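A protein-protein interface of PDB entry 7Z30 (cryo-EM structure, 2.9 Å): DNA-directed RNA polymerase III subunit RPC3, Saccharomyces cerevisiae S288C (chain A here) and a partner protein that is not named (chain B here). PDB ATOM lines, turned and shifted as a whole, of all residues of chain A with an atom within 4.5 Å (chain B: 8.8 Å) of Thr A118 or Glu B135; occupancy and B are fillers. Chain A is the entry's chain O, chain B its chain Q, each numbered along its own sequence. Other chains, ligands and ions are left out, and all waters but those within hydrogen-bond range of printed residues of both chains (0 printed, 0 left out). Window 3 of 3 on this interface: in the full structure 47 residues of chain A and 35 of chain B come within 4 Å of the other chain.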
ATOM      1  N   SER A  75      28.676  -8.393 -14.938  1.00  0.00           N
ATOM      2  CA  SER A  75      28.774  -9.681 -15.604  1.00  0.00           C
ATOM      3  C   SER A  75      30.235 -10.044 -15.860  1.00  0.00           C
ATOM      4  O   SER A  75      31.163  -9.348 -15.442  1.00  0.00           O
ATOM      5  CB  SER A  75      27.982  -9.668 -16.910  1.00  0.00           C
ATOM      6  OG  SER A  75      27.984 -10.949 -17.514  1.00  0.00           O
ATOM      7  N   LYS A  92      37.318 -16.884 -16.509  1.00  0.00           N
ATOM      8  CA  LYS A  92      36.450 -18.005 -16.159  1.00  0.00           C
ATOM      9  C   LYS A  92      37.054 -18.839 -15.035  1.00  0.00           C
ATOM     10  O   LYS A  92      36.366 -19.191 -14.071  1.00  0.00           O
ATOM     11  CB  LYS A  92      36.196 -18.873 -17.392  1.00  0.00           C
ATOM     12  CG  LYS A  92      34.798 -19.467 -17.482  1.00  0.00           C
ATOM     13  CD  LYS A  92      33.714 -18.401 -17.477  1.00  0.00           C
ATOM     14  CE  LYS A  92      33.646 -17.678 -18.809  1.00  0.00           C
ATOM     15  NZ  LYS A  92      32.645 -16.578 -18.784  1.00  0.00           N
ATOM     16  N   LEU A 107      23.715 -14.663 -10.324  1.00  0.00           N
ATOM     17  CA  LEU A 107      22.303 -14.672 -10.681  1.00  0.00           C
ATOM     18  C   LEU A 107      22.173 -14.708 -12.195  1.00  0.00           C
ATOM     19  O   LEU A 107      23.091 -14.309 -12.913  1.00  0.00           O
ATOM     20  CB  LEU A 107      21.559 -13.456 -10.119  1.00  0.00           C
ATOM     21  CG  LEU A 107      20.795 -13.656  -8.811  1.00  0.00           C
ATOM     22  CD1 LEU A 107      19.686 -12.627  -8.690  1.00  0.00           C
ATOM     23  CD2 LEU A 107      20.223 -15.065  -8.739  1.00  0.00           C
ATOM     24  N   GLN A 108      21.024 -15.187 -12.666  1.00  0.00           N
ATOM     25  CA  GLN A 108      20.723 -15.272 -14.092  1.00  0.00           C
ATOM     26  C   GLN A 108      19.414 -14.529 -14.338  1.00  0.00           C
ATOM     27  O   GLN A 108      18.330 -15.113 -14.250  1.00  0.00           O
ATOM     28  CB  GLN A 108      20.629 -16.726 -14.544  1.00  0.00           C
ATOM     29  CG  GLN A 108      21.824 -17.584 -14.164  1.00  0.00           C
ATOM     30  CD  GLN A 108      21.991 -18.783 -15.077  1.00  0.00           C
ATOM     31  OE1 GLN A 108      21.871 -18.669 -16.296  1.00  0.00           O
ATOM     32  NE2 GLN A 108      22.269 -19.942 -14.490  1.00  0.00           N
ATOM     33  N   LYS A 116      19.903 -14.220 -22.758  1.00  0.00           N
ATOM     34  CA  LYS A 116      20.138 -14.050 -21.333  1.00  0.00           C
ATOM     35  C   LYS A 116      21.627 -14.195 -21.036  1.00  0.00           C
ATOM     36  O   LYS A 116      22.314 -15.049 -21.602  1.00  0.00           O
ATOM     37  CB  LYS A 116      19.296 -15.073 -20.545  1.00  0.00           C
ATOM     38  CG  LYS A 116      19.433 -15.165 -19.003  1.00  0.00           C
ATOM     39  CD  LYS A 116      20.774 -15.667 -18.473  1.00  0.00           C
ATOM     40  CE  LYS A 116      21.120 -17.032 -19.046  1.00  0.00           C
ATOM     41  NZ  LYS A 116      22.262 -17.664 -18.325  1.00  0.00           N
ATOM     42  N   THR A 117      22.117 -13.345 -20.135  1.00  0.00           N
ATOM     43  CA  THR A 117      23.475 -13.448 -19.619  1.00  0.00           C
ATOM     44  C   THR A 117      23.429 -13.372 -18.101  1.00  0.00           C
ATOM     45  O   THR A 117      22.670 -12.588 -17.528  1.00  0.00           O
ATOM     46  CB  THR A 117      24.393 -12.345 -20.167  1.00  0.00           C
ATOM     47  OG1 THR A 117      25.597 -12.299 -19.392  1.00  0.00           O
ATOM     48  CG2 THR A 117      23.704 -10.990 -20.096  1.00  0.00           C
ATOM     49  N   THR A 118      24.240 -14.202 -17.453  1.00  0.00           N
ATOM     50  CA  THR A 118      24.271 -14.253 -15.999  1.00  0.00           C
ATOM     51  C   THR A 118      25.167 -13.153 -15.438  1.00  0.00           C
ATOM     52  O   THR A 118      26.192 -12.792 -16.026  1.00  0.00           O
ATOM     53  CB  THR A 118      24.739 -15.628 -15.510  1.00  0.00           C
ATOM     54  OG1 THR A 118      24.566 -15.723 -14.091  1.00  0.00           O
ATOM     55  CG2 THR A 118      26.199 -15.876 -15.862  1.00  0.00           C
ATOM     56  N   TYR A 119      24.754 -12.603 -14.299  1.00  0.00           N
ATOM     57  CA  TYR A 119      25.494 -11.554 -13.614  1.00  0.00           C
ATOM     58  C   TYR A 119      26.148 -12.128 -12.359  1.00  0.00           C
ATOM     59  O   TYR A 119      25.954 -13.292 -12.002  1.00  0.00           O
ATOM     60  CB  TYR A 119      24.583 -10.368 -13.284  1.00  0.00           C
ATOM     61  CG  TYR A 119      23.974  -9.679 -14.491  1.00  0.00           C
ATOM     62  CD1 TYR A 119      23.095 -10.346 -15.338  1.00  0.00           C
ATOM     63  CD2 TYR A 119      24.277  -8.353 -14.778  1.00  0.00           C
ATOM     64  CE1 TYR A 119      22.541  -9.717 -16.433  1.00  0.00           C
ATOM     65  CE2 TYR A 119      23.726  -7.716 -15.874  1.00  0.00           C
ATOM     66  CZ  TYR A 119      22.859  -8.405 -16.698  1.00  0.00           C
ATOM     67  OH  TYR A 119      22.304  -7.782 -17.792  1.00  0.00           O
ATOM     68  N   TYR A 120      26.933 -11.296 -11.679  1.00  0.00           N
ATOM     69  CA  TYR A 120      27.786 -11.792 -10.604  1.00  0.00           C
ATOM     70  C   TYR A 120      27.838 -10.776  -9.475  1.00  0.00           C
ATOM     71  O   TYR A 120      28.165  -9.608  -9.704  1.00  0.00           O
ATOM     72  CB  TYR A 120      29.194 -12.075 -11.130  1.00  0.00           C
ATOM     73  CG  TYR A 120      29.387 -13.489 -11.625  1.00  0.00           C
ATOM     74  CD1 TYR A 120      28.921 -13.877 -12.874  1.00  0.00           C
ATOM     75  CD2 TYR A 120      30.054 -14.428 -10.856  1.00  0.00           C
ATOM     76  CE1 TYR A 120      29.102 -15.168 -13.334  1.00  0.00           C
ATOM     77  CE2 TYR A 120      30.238 -15.720 -11.305  1.00  0.00           C
ATOM     78  CZ  TYR A 120      29.763 -16.083 -12.544  1.00  0.00           C
ATOM     79  OH  TYR A 120      29.949 -17.369 -12.993  1.00  0.00           O
ATOM     80  N   PHE B 132      27.205 -24.344  -9.744  1.00  0.00           N
ATOM     81  CA  PHE B 132      28.025 -23.519 -10.612  1.00  0.00           C
ATOM     82  C   PHE B 132      27.219 -23.058 -11.819  1.00  0.00           C
ATOM     83  O   PHE B 132      26.384 -23.805 -12.339  1.00  0.00           O
ATOM     84  CB  PHE B 132      29.275 -24.268 -11.093  1.00  0.00           C
ATOM     85  CG  PHE B 132      30.314 -24.467 -10.026  1.00  0.00           C
ATOM     86  CD1 PHE B 132      30.314 -23.686  -8.884  1.00  0.00           C
ATOM     87  CD2 PHE B 132      31.304 -25.420 -10.178  1.00  0.00           C
ATOM     88  CE1 PHE B 132      31.271 -23.865  -7.906  1.00  0.00           C
ATOM     89  CE2 PHE B 132      32.266 -25.598  -9.205  1.00  0.00           C
ATOM     90  CZ  PHE B 132      32.249 -24.821  -8.068  1.00  0.00           C
ATOM     91  N   PRO B 133      27.445 -21.831 -12.282  1.00  0.00           N
ATOM     92  CA  PRO B 133      26.697 -21.325 -13.436  1.00  0.00           C
ATOM     93  C   PRO B 133      27.038 -22.086 -14.707  1.00  0.00           C
ATOM     94  O   PRO B 133      28.054 -22.779 -14.805  1.00  0.00           O
ATOM     95  CB  PRO B 133      27.134 -19.858 -13.538  1.00  0.00           C
ATOM     96  CG  PRO B 133      27.744 -19.534 -12.215  1.00  0.00           C
ATOM     97  CD  PRO B 133      28.315 -20.805 -11.686  1.00  0.00           C
ATOM     98  N   ASN B 134      26.152 -21.945 -15.695  1.00  0.00           N
ATOM     99  CA  ASN B 134      26.328 -22.644 -16.962  1.00  0.00           C
ATOM    100  C   ASN B 134      27.582 -22.179 -17.693  1.00  0.00           C
ATOM    101  O   ASN B 134      28.218 -22.973 -18.396  1.00  0.00           O
ATOM    102  CB  ASN B 134      25.095 -22.445 -17.841  1.00  0.00           C
ATOM    103  CG  ASN B 134      23.847 -23.062 -17.242  1.00  0.00           C
ATOM    104  OD1 ASN B 134      22.950 -22.355 -16.783  1.00  0.00           O
ATOM    105  ND2 ASN B 134      23.783 -24.388 -17.243  1.00  0.00           N
ATOM    106  N   GLU B 135      27.948 -20.903 -17.546  1.00  0.00           N
ATOM    107  CA  GLU B 135      29.139 -20.395 -18.218  1.00  0.00           C
ATOM    108  C   GLU B 135      30.413 -20.986 -17.629  1.00  0.00           C
ATOM    109  O   GLU B 135      31.458 -20.987 -18.288  1.00  0.00           O
ATOM    110  CB  GLU B 135      29.180 -18.869 -18.137  1.00  0.00           C
ATOM    111  CG  GLU B 135      27.817 -18.207 -18.226  1.00  0.00           C
ATOM    112  CD  GLU B 135      27.444 -17.828 -19.644  1.00  0.00           C
ATOM    113  OE1 GLU B 135      28.223 -18.141 -20.569  1.00  0.00           O
ATOM    114  OE2 GLU B 135      26.369 -17.221 -19.834  1.00  0.00           O
ATOM    115  N   LEU B 136      30.351 -21.484 -16.397  1.00  0.00           N
ATOM    116  CA  LEU B 136      31.507 -22.072 -15.734  1.00  0.00           C
ATOM    117  C   LEU B 136      31.634 -23.570 -15.985  1.00  0.00           C
ATOM    118  O   LEU B 136      32.618 -24.176 -15.545  1.00  0.00           O
ATOM    119  CB  LEU B 136      31.440 -21.801 -14.226  1.00  0.00           C
ATOM    120  CG  LEU B 136      31.766 -20.369 -13.791  1.00  0.00           C
ATOM    121  CD1 LEU B 136      31.737 -20.226 -12.279  1.00  0.00           C
ATOM    122  CD2 LEU B 136      33.114 -19.944 -14.330  1.00  0.00           C
ATOM    123  N   TYR B 137      30.669 -24.178 -16.680  1.00  0.00           N
ATOM    124  CA  TYR B 137      30.721 -25.609 -16.954  1.00  0.00           C
ATOM    125  C   TYR B 137      31.803 -25.967 -17.964  1.00  0.00           C
ATOM    126  O   TYR B 137      32.400 -27.044 -17.866  1.00  0.00           O
ATOM    127  CB  TYR B 137      29.368 -26.098 -17.471  1.00  0.00           C
ATOM    128  CG  TYR B 137      28.321 -26.291 -16.403  1.00  0.00           C
ATOM    129  CD1 TYR B 137      28.663 -26.303 -15.058  1.00  0.00           C
ATOM    130  CD2 TYR B 137      26.988 -26.470 -16.743  1.00  0.00           C
ATOM    131  CE1 TYR B 137      27.701 -26.481 -14.081  1.00  0.00           C
ATOM    132  CE2 TYR B 137      26.023 -26.649 -15.776  1.00  0.00           C
ATOM    133  CZ  TYR B 137      26.384 -26.654 -14.449  1.00  0.00           C
ATOM    134  OH  TYR B 137      25.416 -26.833 -13.491  1.00  0.00           O
ATOM    135  N   ASN B 138      32.064 -25.088 -18.935  1.00  0.00           N
ATOM    136  CA  ASN B 138      33.014 -25.395 -19.998  1.00  0.00           C
ATOM    137  C   ASN B 138      34.427 -25.609 -19.474  1.00  0.00           C
ATOM    138  O   ASN B 138      35.129 -26.498 -19.970  1.00  0.00           O
ATOM    139  CB  ASN B 138      33.023 -24.276 -21.037  1.00  0.00           C
ATOM    140  CG  ASN B 138      33.245 -22.913 -20.418  1.00  0.00           C
ATOM    141  OD1 ASN B 138      33.324 -22.780 -19.197  1.00  0.00           O
ATOM    142  ND2 ASN B 138      33.356 -21.891 -21.258  1.00  0.00           N
ATOM    143  N   VAL B 139      34.859 -24.815 -18.495  1.00  0.00           N
ATOM    144  CA  VAL B 139      36.191 -24.989 -17.927  1.00  0.00           C
ATOM    145  C   VAL B 139      36.303 -26.345 -17.239  1.00  0.00           C
ATOM    146  O   VAL B 139      37.388 -26.934 -17.171  1.00  0.00           O
ATOM    147  CB  VAL B 139      36.501 -23.819 -16.972  1.00  0.00           C
ATOM    148  CG1 VAL B 139      37.550 -24.198 -15.930  1.00  0.00           C
ATOM    149  CG2 VAL B 139      36.948 -22.596 -17.761  1.00  0.00           C
ATOM    150  N   MET B 140      35.181 -26.883 -16.772  1.00  0.00           N
ATOM    151  CA  MET B 140      35.197 -28.136 -16.033  1.00  0.00           C
ATOM    152  C   MET B 140      35.149 -29.331 -16.979  1.00  0.00           C
ATOM    153  O   MET B 140      34.672 -29.232 -18.112  1.00  0.00           O
ATOM    154  CB  MET B 140      34.018 -28.190 -15.065  1.00  0.00           C
ATOM    155  CG  MET B 140      34.319 -28.943 -13.786  1.00  0.00           C
ATOM    156  SD  MET B 140      35.069 -27.861 -12.561  1.00  0.00           S
ATOM    157  CE  MET B 140      34.147 -26.349 -12.825  1.00  0.00           C
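Among the printed residues, merely in contact across the chains: Tyr A120 with Pro B133 (3.2 Å), Lys A92 with Leu B136 (3.3 Å), Tyr A120 with Leu B136 (3.4 Å), Lys A92 with Glu B135 (3.5 Å), Thr A118 with Glu B135 (3.7 Å) and Lys A92 with Val B139 (3.8 Å).
Of chain B, only Glu B135 (3.7 Å) comes within 4 Å of Thr A118.
Of chain A, only Lys A92 and Thr A118 come within 4 Å of Glu B135.
Of the printed residues of chain A, Leu B136 touches Lys A92 and Tyr A120.
Printed residues of chain A within 4 Å of Val B139: Lys A92 (3.8 Å).
Printed residues of chain B within 4 Å of Lys A92: Glu B135, Leu B136 and Val B139.
Of the printed residues of chain A, Asn B134 touches Gln A108 (3.4 Å).
Printed residues of chain B within 4 Å of Gln A108: Asn B134.
The nearest residue of chain A that does not touch Glu B135 is Lys A116 (4.4 Å).
Along chain A the printed residues that touch a printed residue of chain B span positions 92 to 120.
Of the 9 printed residues of chain B, 5 touch a printed residue of chain A.
Printed residues of chain B that touch a printed residue of chain A: Pro B133, Asn B134, Glu B135, Leu B136 and Val B139.
Hydrophobic or aromatic side chains of chain B that line the printed part of chain A: Pro B133, Leu B136 and Val B139.
Among the printed residues, no Asp or Glu carboxylate lies within 4 Å of a Lys or Arg side-chain nitrogen of the other chain.
The side-chain amide nitrogen of Gln A108 is in hydrogen-bond range of the side-chain amide oxygen of Asn B134 (3.4 Å).
The backbone carbonyl oxygen of Thr A118 is in hydrogen-bond range of the side-chain hydroxyl of Ser A75.
OD1 of Asn B138 sits close to O of Glu B135 (2.7 Å).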
